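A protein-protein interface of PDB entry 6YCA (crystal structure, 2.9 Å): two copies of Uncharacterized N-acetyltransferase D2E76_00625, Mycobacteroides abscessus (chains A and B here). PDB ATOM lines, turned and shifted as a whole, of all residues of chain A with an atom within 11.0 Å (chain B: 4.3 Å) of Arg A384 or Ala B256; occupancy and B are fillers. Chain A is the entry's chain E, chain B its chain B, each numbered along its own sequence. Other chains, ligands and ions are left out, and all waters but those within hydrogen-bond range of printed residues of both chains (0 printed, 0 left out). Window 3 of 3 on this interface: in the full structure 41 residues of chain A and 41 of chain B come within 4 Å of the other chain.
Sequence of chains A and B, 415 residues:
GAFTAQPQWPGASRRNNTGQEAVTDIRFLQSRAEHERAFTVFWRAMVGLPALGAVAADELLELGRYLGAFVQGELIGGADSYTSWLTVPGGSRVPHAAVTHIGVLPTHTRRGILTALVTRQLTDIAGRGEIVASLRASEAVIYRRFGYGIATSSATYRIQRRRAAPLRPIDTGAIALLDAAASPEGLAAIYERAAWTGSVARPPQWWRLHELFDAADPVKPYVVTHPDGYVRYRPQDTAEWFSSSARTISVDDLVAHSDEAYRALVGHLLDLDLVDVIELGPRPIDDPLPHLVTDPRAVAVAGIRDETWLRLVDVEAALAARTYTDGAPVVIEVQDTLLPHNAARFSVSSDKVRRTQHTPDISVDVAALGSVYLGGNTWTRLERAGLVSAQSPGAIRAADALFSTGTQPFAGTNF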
ATOM      1  N   ILE A 362     -13.569  -5.900   6.318  1.00  0.00           N
ATOM      2  CA  ILE A 362     -14.503  -5.697   5.219  1.00  0.00           C
ATOM      3  C   ILE A 362     -15.806  -6.402   5.572  1.00  0.00           C
ATOM      4  O   ILE A 362     -15.798  -7.508   6.121  1.00  0.00           O
ATOM      5  CB  ILE A 362     -13.905  -6.218   3.891  1.00  0.00           C
ATOM      6  CG1 ILE A 362     -12.936  -5.192   3.302  1.00  0.00           C
ATOM      7  CG2 ILE A 362     -14.992  -6.585   2.894  1.00  0.00           C
ATOM      8  CD1 ILE A 362     -12.231  -5.672   2.059  1.00  0.00           C
ATOM      9  N   SER A 363     -16.925  -5.746   5.276  1.00  0.00           N
ATOM     10  CA  SER A 363     -18.250  -6.324   5.450  1.00  0.00           C
ATOM     11  C   SER A 363     -18.939  -6.308   4.093  1.00  0.00           C
ATOM     12  O   SER A 363     -18.960  -5.275   3.416  1.00  0.00           O
ATOM     13  CB  SER A 363     -19.060  -5.529   6.478  1.00  0.00           C
ATOM     14  OG  SER A 363     -20.224  -6.232   6.874  1.00  0.00           O
ATOM     15  N   VAL A 364     -19.491  -7.451   3.693  1.00  0.00           N
ATOM     16  CA  VAL A 364     -20.069  -7.600   2.363  1.00  0.00           C
ATOM     17  C   VAL A 364     -21.119  -8.701   2.405  1.00  0.00           C
ATOM     18  O   VAL A 364     -21.028  -9.639   3.201  1.00  0.00           O
ATOM     19  CB  VAL A 364     -18.953  -7.888   1.327  1.00  0.00           C
ATOM     20  CG1 VAL A 364     -18.358  -9.276   1.537  1.00  0.00           C
ATOM     21  CG2 VAL A 364     -19.463  -7.718  -0.084  1.00  0.00           C
ATOM     22  N   ALA A 368     -22.167 -10.263  -3.385  1.00  0.00           N
ATOM     23  CA  ALA A 368     -21.008  -9.519  -3.863  1.00  0.00           C
ATOM     24  C   ALA A 368     -19.716 -10.290  -3.631  1.00  0.00           C
ATOM     25  O   ALA A 368     -18.781 -10.178  -4.430  1.00  0.00           O
ATOM     26  CB  ALA A 368     -20.952  -8.139  -3.212  1.00  0.00           C
ATOM     27  N   VAL A 372     -16.598 -11.433  -6.468  1.00  0.00           N
ATOM     28  CA  VAL A 372     -15.144 -11.352  -6.341  1.00  0.00           C
ATOM     29  C   VAL A 372     -14.478 -12.724  -6.339  1.00  0.00           C
ATOM     30  O   VAL A 372     -13.284 -12.828  -6.655  1.00  0.00           O
ATOM     31  CB  VAL A 372     -14.751 -10.560  -5.082  1.00  0.00           C
ATOM     32  CG1 VAL A 372     -13.254 -10.291  -5.051  1.00  0.00           C
ATOM     33  CG2 VAL A 372     -15.507  -9.252  -5.029  1.00  0.00           C
ATOM     34  N   ASN A 377     -14.096  -9.653 -10.515  1.00  0.00           N
ATOM     35  CA  ASN A 377     -14.322  -8.328  -9.964  1.00  0.00           C
ATOM     36  C   ASN A 377     -13.336  -8.114  -8.831  1.00  0.00           C
ATOM     37  O   ASN A 377     -12.845  -9.070  -8.224  1.00  0.00           O
ATOM     38  CB  ASN A 377     -15.748  -8.184  -9.437  1.00  0.00           C
ATOM     39  CG  ASN A 377     -16.769  -8.253 -10.536  1.00  0.00           C
ATOM     40  OD1 ASN A 377     -17.518  -9.223 -10.636  1.00  0.00           O
ATOM     41  ND2 ASN A 377     -16.805  -7.227 -11.376  1.00  0.00           N
ATOM     42  N   THR A 378     -13.066  -6.848  -8.538  1.00  0.00           N
ATOM     43  CA  THR A 378     -12.153  -6.487  -7.466  1.00  0.00           C
ATOM     44  C   THR A 378     -12.909  -5.825  -6.326  1.00  0.00           C
ATOM     45  O   THR A 378     -14.044  -5.364  -6.481  1.00  0.00           O
ATOM     46  CB  THR A 378     -11.046  -5.552  -7.971  1.00  0.00           C
ATOM     47  OG1 THR A 378     -11.627  -4.339  -8.460  1.00  0.00           O
ATOM     48  CG2 THR A 378     -10.256  -6.213  -9.086  1.00  0.00           C
ATOM     49  N   TRP A 379     -12.260  -5.785  -5.165  1.00  0.00           N
ATOM     50  CA  TRP A 379     -12.887  -5.165  -4.005  1.00  0.00           C
ATOM     51  C   TRP A 379     -13.019  -3.659  -4.169  1.00  0.00           C
ATOM     52  O   TRP A 379     -13.981  -3.070  -3.662  1.00  0.00           O
ATOM     53  CB  TRP A 379     -12.126  -5.519  -2.732  1.00  0.00           C
ATOM     54  CG  TRP A 379     -12.230  -6.961  -2.360  1.00  0.00           C
ATOM     55  CD1 TRP A 379     -11.299  -7.935  -2.567  1.00  0.00           C
ATOM     56  CD2 TRP A 379     -13.335  -7.593  -1.706  1.00  0.00           C
ATOM     57  NE1 TRP A 379     -11.754  -9.137  -2.076  1.00  0.00           N
ATOM     58  CE2 TRP A 379     -13.002  -8.953  -1.542  1.00  0.00           C
ATOM     59  CE3 TRP A 379     -14.574  -7.138  -1.236  1.00  0.00           C
ATOM     60  CZ2 TRP A 379     -13.863  -9.865  -0.933  1.00  0.00           C
ATOM     61  CZ3 TRP A 379     -15.429  -8.045  -0.631  1.00  0.00           C
ATOM     62  CH2 TRP A 379     -15.069  -9.393  -0.486  1.00  0.00           C
ATOM     63  N   THR A 380     -12.074  -3.019  -4.866  1.00  0.00           N
ATOM     64  CA  THR A 380     -12.161  -1.576  -5.054  1.00  0.00           C
ATOM     65  C   THR A 380     -13.378  -1.207  -5.890  1.00  0.00           C
ATOM     66  O   THR A 380     -14.098  -0.256  -5.562  1.00  0.00           O
ATOM     67  CB  THR A 380     -10.887  -1.037  -5.706  1.00  0.00           C
ATOM     68  OG1 THR A 380      -9.737  -1.544  -5.018  1.00  0.00           O
ATOM     69  CG2 THR A 380     -10.866   0.490  -5.648  1.00  0.00           C
ATOM     70  N   ARG A 381     -13.630  -1.949  -6.972  1.00  0.00           N
ATOM     71  CA  ARG A 381     -14.737  -1.584  -7.849  1.00  0.00           C
ATOM     72  C   ARG A 381     -16.093  -1.884  -7.223  1.00  0.00           C
ATOM     73  O   ARG A 381     -17.042  -1.117  -7.418  1.00  0.00           O
ATOM     74  CB  ARG A 381     -14.577  -2.194  -9.244  1.00  0.00           C
ATOM     75  CG  ARG A 381     -13.409  -1.595 -10.033  1.00  0.00           C
ATOM     76  CD  ARG A 381     -13.557  -0.071 -10.178  1.00  0.00           C
ATOM     77  NE  ARG A 381     -12.569   0.526 -11.079  1.00  0.00           N
ATOM     78  CZ  ARG A 381     -12.383   1.837 -11.221  1.00  0.00           C
ATOM     79  NH1 ARG A 381     -13.115   2.691 -10.520  1.00  0.00           N
ATOM     80  NH2 ARG A 381     -11.465   2.299 -12.061  1.00  0.00           N
ATOM     81  N   LEU A 382     -16.206  -2.966  -6.452  1.00  0.00           N
ATOM     82  CA  LEU A 382     -17.473  -3.234  -5.781  1.00  0.00           C
ATOM     83  C   LEU A 382     -17.727  -2.237  -4.660  1.00  0.00           C
ATOM     84  O   LEU A 382     -18.876  -1.847  -4.419  1.00  0.00           O
ATOM     85  CB  LEU A 382     -17.530  -4.671  -5.273  1.00  0.00           C
ATOM     86  CG  LEU A 382     -17.809  -5.696  -6.374  1.00  0.00           C
ATOM     87  CD1 LEU A 382     -18.068  -7.062  -5.781  1.00  0.00           C
ATOM     88  CD2 LEU A 382     -18.987  -5.256  -7.224  1.00  0.00           C
ATOM     89  N   GLU A 383     -16.672  -1.815  -3.963  1.00  0.00           N
ATOM     90  CA  GLU A 383     -16.829  -0.753  -2.978  1.00  0.00           C
ATOM     91  C   GLU A 383     -17.293   0.540  -3.637  1.00  0.00           C
ATOM     92  O   GLU A 383     -18.117   1.271  -3.074  1.00  0.00           O
ATOM     93  CB  GLU A 383     -15.512  -0.526  -2.243  1.00  0.00           C
ATOM     94  CG  GLU A 383     -15.608   0.531  -1.167  1.00  0.00           C
ATOM     95  CD  GLU A 383     -14.264   1.089  -0.785  1.00  0.00           C
ATOM     96  OE1 GLU A 383     -13.340   1.034  -1.628  1.00  0.00           O
ATOM     97  OE2 GLU A 383     -14.130   1.576   0.360  1.00  0.00           O
ATOM     98  N   ARG A 384     -16.784   0.830  -4.842  1.00  0.00           N
ATOM     99  CA  ARG A 384     -17.185   2.042  -5.552  1.00  0.00           C
ATOM    100  C   ARG A 384     -18.672   2.031  -5.873  1.00  0.00           C
ATOM    101  O   ARG A 384     -19.333   3.076  -5.835  1.00  0.00           O
ATOM    102  CB  ARG A 384     -16.374   2.186  -6.837  1.00  0.00           C
ATOM    103  CG  ARG A 384     -16.533   3.530  -7.534  1.00  0.00           C
ATOM    104  CD  ARG A 384     -15.328   3.853  -8.407  1.00  0.00           C
ATOM    105  NE  ARG A 384     -15.364   5.218  -8.924  1.00  0.00           N
ATOM    106  CZ  ARG A 384     -14.768   6.249  -8.345  1.00  0.00           C
ATOM    107  NH1 ARG A 384     -14.090   6.078  -7.222  1.00  0.00           N
ATOM    108  NH2 ARG A 384     -14.854   7.453  -8.886  1.00  0.00           N
ATOM    109  N   ALA A 385     -19.219   0.860  -6.179  1.00  0.00           N
ATOM    110  CA  ALA A 385     -20.645   0.738  -6.431  1.00  0.00           C
ATOM    111  C   ALA A 385     -21.469   0.743  -5.154  1.00  0.00           C
ATOM    112  O   ALA A 385     -22.702   0.737  -5.237  1.00  0.00           O
ATOM    113  CB  ALA A 385     -20.926  -0.544  -7.214  1.00  0.00           C
ATOM    114  N   GLY A 386     -20.831   0.765  -3.987  1.00  0.00           N
ATOM    115  CA  GLY A 386     -21.548   0.781  -2.729  1.00  0.00           C
ATOM    116  C   GLY A 386     -21.943  -0.576  -2.191  1.00  0.00           C
ATOM    117  O   GLY A 386     -22.866  -0.655  -1.374  1.00  0.00           O
ATOM    118  N   LEU A 387     -21.273  -1.647  -2.615  1.00  0.00           N
ATOM    119  CA  LEU A 387     -21.589  -2.998  -2.177  1.00  0.00           C
ATOM    120  C   LEU A 387     -20.589  -3.553  -1.174  1.00  0.00           C
ATOM    121  O   LEU A 387     -20.727  -4.711  -0.762  1.00  0.00           O
ATOM    122  CB  LEU A 387     -21.674  -3.944  -3.376  1.00  0.00           C
ATOM    123  CG  LEU A 387     -22.777  -3.683  -4.395  1.00  0.00           C
ATOM    124  CD1 LEU A 387     -22.582  -4.560  -5.607  1.00  0.00           C
ATOM    125  CD2 LEU A 387     -24.128  -3.942  -3.769  1.00  0.00           C
ATOM    126  N   VAL A 388     -19.588  -2.772  -0.777  1.00  0.00           N
ATOM    127  CA  VAL A 388     -18.565  -3.220   0.162  1.00  0.00           C
ATOM    128  C   VAL A 388     -18.311  -2.109   1.171  1.00  0.00           C
ATOM    129  O   VAL A 388     -18.175  -0.941   0.791  1.00  0.00           O
ATOM    130  CB  VAL A 388     -17.256  -3.603  -0.557  1.00  0.00           C
ATOM    131  CG1 VAL A 388     -16.193  -4.009   0.450  1.00  0.00           C
ATOM    132  CG2 VAL A 388     -17.501  -4.729  -1.547  1.00  0.00           C
ATOM    133  N   SER A 389     -18.245  -2.470   2.452  1.00  0.00           N
ATOM    134  CA  SER A 389     -17.955  -1.528   3.522  1.00  0.00           C
ATOM    135  C   SER A 389     -16.574  -1.855   4.073  1.00  0.00           C
ATOM    136  O   SER A 389     -16.345  -2.960   4.577  1.00  0.00           O
ATOM    137  CB  SER A 389     -19.003  -1.654   4.628  1.00  0.00           C
ATOM    138  OG  SER A 389     -18.658  -0.872   5.760  1.00  0.00           O
ATOM    139  N   ALA A 390     -15.671  -0.883   3.996  1.00  0.00           N
ATOM    140  CA  ALA A 390     -14.282  -1.004   4.413  1.00  0.00           C
ATOM    141  C   ALA A 390     -14.029  -0.222   5.693  1.00  0.00           C
ATOM    142  O   ALA A 390     -14.653   0.813   5.942  1.00  0.00           O
ATOM    143  CB  ALA A 390     -13.331  -0.505   3.324  1.00  0.00           C
ATOM    144  N   PRO A 393      -9.011   2.620   4.094  1.00  0.00           N
ATOM    145  CA  PRO A 393      -8.821   2.632   2.635  1.00  0.00           C
ATOM    146  C   PRO A 393      -7.815   1.593   2.179  1.00  0.00           C
ATOM    147  O   PRO A 393      -7.883   1.135   1.031  1.00  0.00           O
ATOM    148  CB  PRO A 393      -8.356   4.065   2.340  1.00  0.00           C
ATOM    149  CG  PRO A 393      -7.817   4.567   3.641  1.00  0.00           C
ATOM    150  CD  PRO A 393      -8.651   3.911   4.706  1.00  0.00           C
ATOM    151  N   ILE A 396      -9.081  -2.313   1.606  1.00  0.00           N
ATOM    152  CA  ILE A 396      -9.477  -2.667   0.249  1.00  0.00           C
ATOM    153  C   ILE A 396      -8.250  -3.092  -0.549  1.00  0.00           C
ATOM    154  O   ILE A 396      -8.278  -4.086  -1.283  1.00  0.00           O
ATOM    155  CB  ILE A 396     -10.210  -1.480  -0.403  1.00  0.00           C
ATOM    156  CG1 ILE A 396     -11.548  -1.242   0.296  1.00  0.00           C
ATOM    157  CG2 ILE A 396     -10.438  -1.715  -1.884  1.00  0.00           C
ATOM    158  CD1 ILE A 396     -12.541  -2.370   0.133  1.00  0.00           C
ATOM    159  N   ASP A 400      -7.649  -6.808  -2.097  1.00  0.00           N
ATOM    160  CA  ASP A 400      -7.387  -6.992  -3.518  1.00  0.00           C
ATOM    161  C   ASP A 400      -6.020  -7.613  -3.762  1.00  0.00           C
ATOM    162  O   ASP A 400      -5.856  -8.372  -4.721  1.00  0.00           O
ATOM    163  CB  ASP A 400      -7.523  -5.665  -4.254  1.00  0.00           C
ATOM    164  CG  ASP A 400      -8.963  -5.322  -4.547  1.00  0.00           C
ATOM    165  OD1 ASP A 400      -9.753  -6.258  -4.802  1.00  0.00           O
ATOM    166  OD2 ASP A 400      -9.305  -4.121  -4.516  1.00  0.00           O
ATOM    167  N   ASP B 228     -16.928  16.746  -4.800  1.00  0.00           N
ATOM    168  CA  ASP B 228     -15.726  16.006  -5.173  1.00  0.00           C
ATOM    169  C   ASP B 228     -15.744  15.563  -6.631  1.00  0.00           C
ATOM    170  O   ASP B 228     -15.150  14.538  -6.972  1.00  0.00           O
ATOM    171  CB  ASP B 228     -15.498  14.802  -4.258  1.00  0.00           C
ATOM    172  CG  ASP B 228     -15.155  15.200  -2.845  1.00  0.00           C
ATOM    173  OD1 ASP B 228     -14.312  16.099  -2.677  1.00  0.00           O
ATOM    174  OD2 ASP B 228     -15.732  14.619  -1.902  1.00  0.00           O
ATOM    175  N   LEU B 254     -16.757  12.604 -17.052  1.00  0.00           N
ATOM    176  CA  LEU B 254     -17.257  12.249 -15.724  1.00  0.00           C
ATOM    177  C   LEU B 254     -16.032  12.160 -14.820  1.00  0.00           C
ATOM    178  O   LEU B 254     -15.294  11.170 -14.861  1.00  0.00           O
ATOM    179  CB  LEU B 254     -18.006  10.921 -15.750  1.00  0.00           C
ATOM    180  CG  LEU B 254     -19.063  10.655 -14.666  1.00  0.00           C
ATOM    181  CD1 LEU B 254     -19.771   9.325 -14.935  1.00  0.00           C
ATOM    182  CD2 LEU B 254     -18.504  10.700 -13.249  1.00  0.00           C
ATOM    183  N   VAL B 255     -15.835  13.179 -13.992  1.00  0.00           N
ATOM    184  CA  VAL B 255     -14.712  13.248 -13.066  1.00  0.00           C
ATOM    185  C   VAL B 255     -15.255  13.052 -11.656  1.00  0.00           C
ATOM    186  O   VAL B 255     -16.120  13.813 -11.204  1.00  0.00           O
ATOM    187  CB  VAL B 255     -13.959  14.579 -13.205  1.00  0.00           C
ATOM    188  CG1 VAL B 255     -12.823  14.648 -12.211  1.00  0.00           C
ATOM    189  CG2 VAL B 255     -13.432  14.730 -14.615  1.00  0.00           C
ATOM    190  N   ALA B 256     -14.760  12.027 -10.965  1.00  0.00           N
ATOM    191  CA  ALA B 256     -15.216  11.708  -9.615  1.00  0.00           C
ATOM    192  C   ALA B 256     -14.019  11.287  -8.782  1.00  0.00           C
ATOM    193  O   ALA B 256     -13.403  10.252  -9.059  1.00  0.00           O
ATOM    194  CB  ALA B 256     -16.260  10.587  -9.638  1.00  0.00           C
ATOM    195  N   HIS B 257     -13.699  12.078  -7.762  1.00  0.00           N
ATOM    196  CA  HIS B 257     -12.553  11.827  -6.901  1.00  0.00           C
ATOM    197  C   HIS B 257     -12.907  11.022  -5.660  1.00  0.00           C
ATOM    198  O   HIS B 257     -12.046  10.823  -4.796  1.00  0.00           O
ATOM    199  CB  HIS B 257     -11.904  13.149  -6.492  1.00  0.00           C
ATOM    200  CG  HIS B 257     -11.616  14.055  -7.644  1.00  0.00           C
ATOM    201  ND1 HIS B 257     -10.756  13.707  -8.661  1.00  0.00           N
ATOM    202  CD2 HIS B 257     -12.083  15.288  -7.947  1.00  0.00           C
ATOM    203  CE1 HIS B 257     -10.699  14.692  -9.539  1.00  0.00           C
ATOM    204  NE2 HIS B 257     -11.497  15.662  -9.130  1.00  0.00           N
ATOM    205  N   SER B 258     -14.140  10.531  -5.567  1.00  0.00           N
ATOM    206  CA  SER B 258     -14.603   9.830  -4.383  1.00  0.00           C
ATOM    207  C   SER B 258     -15.667   8.827  -4.794  1.00  0.00           C
ATOM    208  O   SER B 258     -16.336   9.004  -5.815  1.00  0.00           O
ATOM    209  CB  SER B 258     -15.210  10.835  -3.400  1.00  0.00           C
ATOM    210  OG  SER B 258     -15.874  10.175  -2.349  1.00  0.00           O
ATOM    211  N   ASP B 259     -15.793   7.746  -4.016  1.00  0.00           N
ATOM    212  CA  ASP B 259     -16.878   6.804  -4.269  1.00  0.00           C
ATOM    213  C   ASP B 259     -18.234   7.475  -4.111  1.00  0.00           C
ATOM    214  O   ASP B 259     -19.133   7.273  -4.934  1.00  0.00           O
ATOM    215  CB  ASP B 259     -16.772   5.581  -3.355  1.00  0.00           C
ATOM    216  CG  ASP B 259     -15.657   4.642  -3.761  1.00  0.00           C
ATOM    217  OD1 ASP B 259     -15.122   4.822  -4.875  1.00  0.00           O
ATOM    218  OD2 ASP B 259     -15.319   3.726  -2.973  1.00  0.00           O
ATOM    219  N   ALA B 261     -18.921  10.690  -4.493  1.00  0.00           N
ATOM    220  CA  ALA B 261     -19.108  11.583  -5.630  1.00  0.00           C
ATOM    221  C   ALA B 261     -19.478  10.799  -6.884  1.00  0.00           C
ATOM    222  O   ALA B 261     -20.316  11.239  -7.681  1.00  0.00           O
ATOM    223  CB  ALA B 261     -17.832  12.387  -5.868  1.00  0.00           C
ATOM    224  N   TYR B 262     -18.866   9.626  -7.068  1.00  0.00           N
ATOM    225  CA  TYR B 262     -19.152   8.803  -8.236  1.00  0.00           C
ATOM    226  C   TYR B 262     -20.614   8.387  -8.274  1.00  0.00           C
ATOM    227  O   TYR B 262     -21.271   8.480  -9.318  1.00  0.00           O
ATOM    228  CB  TYR B 262     -18.242   7.579  -8.250  1.00  0.00           C
ATOM    229  CG  TYR B 262     -18.587   6.596  -9.344  1.00  0.00           C
ATOM    230  CD1 TYR B 262     -18.201   6.834 -10.658  1.00  0.00           C
ATOM    231  CD2 TYR B 262     -19.285   5.427  -9.065  1.00  0.00           C
ATOM    232  CE1 TYR B 262     -18.509   5.943 -11.667  1.00  0.00           C
ATOM    233  CE2 TYR B 262     -19.594   4.527 -10.070  1.00  0.00           C
ATOM    234  CZ  TYR B 262     -19.204   4.790 -11.370  1.00  0.00           C
ATOM    235  OH  TYR B 262     -19.506   3.901 -12.380  1.00  0.00           O
ATOM    236  N   ARG B 263     -21.132   7.890  -7.150  1.00  0.00           N
ATOM    237  CA  ARG B 263     -22.518   7.439  -7.115  1.00  0.00           C
ATOM    238  C   ARG B 263     -23.489   8.603  -7.296  1.00  0.00           C
ATOM    239  O   ARG B 263     -24.476   8.483  -8.030  1.00  0.00           O
ATOM    240  CB  ARG B 263     -22.791   6.687  -5.813  1.00  0.00           C
ATOM    241  CG  ARG B 263     -22.027   5.377  -5.697  1.00  0.00           C
ATOM    242  CD  ARG B 263     -22.417   4.598  -4.452  1.00  0.00           C
ATOM    243  NE  ARG B 263     -22.049   5.287  -3.218  1.00  0.00           N
ATOM    244  CZ  ARG B 263     -20.938   5.046  -2.526  1.00  0.00           C
ATOM    245  NH1 ARG B 263     -20.081   4.124  -2.945  1.00  0.00           N
ATOM    246  NH2 ARG B 263     -20.687   5.719  -1.410  1.00  0.00           N
ATOM    247  N   PRO B 288     -17.879   0.413 -12.605  1.00  0.00           N
ATOM    248  CA  PRO B 288     -18.856  -0.460 -11.936  1.00  0.00           C
ATOM    249  C   PRO B 288     -20.315  -0.080 -12.155  1.00  0.00           C
ATOM    250  O   PRO B 288     -21.151  -0.342 -11.285  1.00  0.00           O
ATOM    251  CB  PRO B 288     -18.473  -0.338 -10.456  1.00  0.00           C
ATOM    252  CG  PRO B 288     -17.873   1.035 -10.351  1.00  0.00           C
ATOM    253  CD  PRO B 288     -17.160   1.280 -11.655  1.00  0.00           C
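OD1 of Asp B259 lies within salt-bridge range of NH1 of Arg A384, at 2.9 Å.
O of Arg A384 lies within hydrogen-bond range of NH1 of Arg B263.
The guanidinium group (NH2) of Arg A384 lies within hydrogen-bond range of the backbone carbonyl oxygen (O) of Ala B256, 3.2 Å away.
NH1 of Arg B263 lies within hydrogen-bond range of O of Glu A383 (3.5 Å).
The backbone NH of Arg A381 lies within hydrogen-bond range of the side-chain hydroxyl of Thr A378 (3.5 Å).
Among the printed residues, pairs that only touch across the chains: Arg A381 with Pro B288, Glu A383 with Asp B259, Arg A384 with Ser B258, Arg A384 with Tyr B262, Arg A384 with Pro B288, Ala A385 with Arg B263 and Gly A386 with Arg B263.
Of chain A, only Arg A384 (3.2 Å) comes within 4 Å of Ala B256.
No residue of chain A comes within 4 Å of Leu B254.
His B257 touches none of the printed residues of chain A.
No residue of chain A comes within 4 Å of Ala B261.
Of the printed residues of chain B, Glu A383 touches Asp B259 (3.6 Å) and Arg B263 (3.5 Å).
Of the printed residues of chain B, Arg A381 touches Pro B288.
Of the printed residues of chain B, Gly A386 touches Arg B263.
Printed residues of chain A within 4 Å of Arg B263: Glu A383, Arg A384, Ala A385 and Gly A386.
Ser A363 touches none of the printed residues of chain B.
Pro A393 touches none of the printed residues of chain B.
The nearest printed residue of chain B that does not touch Arg A384 is His B257 (4.9 Å).
The nearest printed residue of chain B that does not touch Gly A386 is Asp B259 (6.3 Å).
Hydrophobic or aromatic side chains of chain B within 4 Å of the printed part of chain A: Ala B256, Tyr B262 and Pro B288.
Among the printed residues, 11 pairs touch across the chains.
Among the printed residues, Asp or Glu carboxylates within 4 Å of a Lys or Arg side-chain nitrogen of the other chain: Arg A384 with Asp B259.
No position is printed for both chains.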
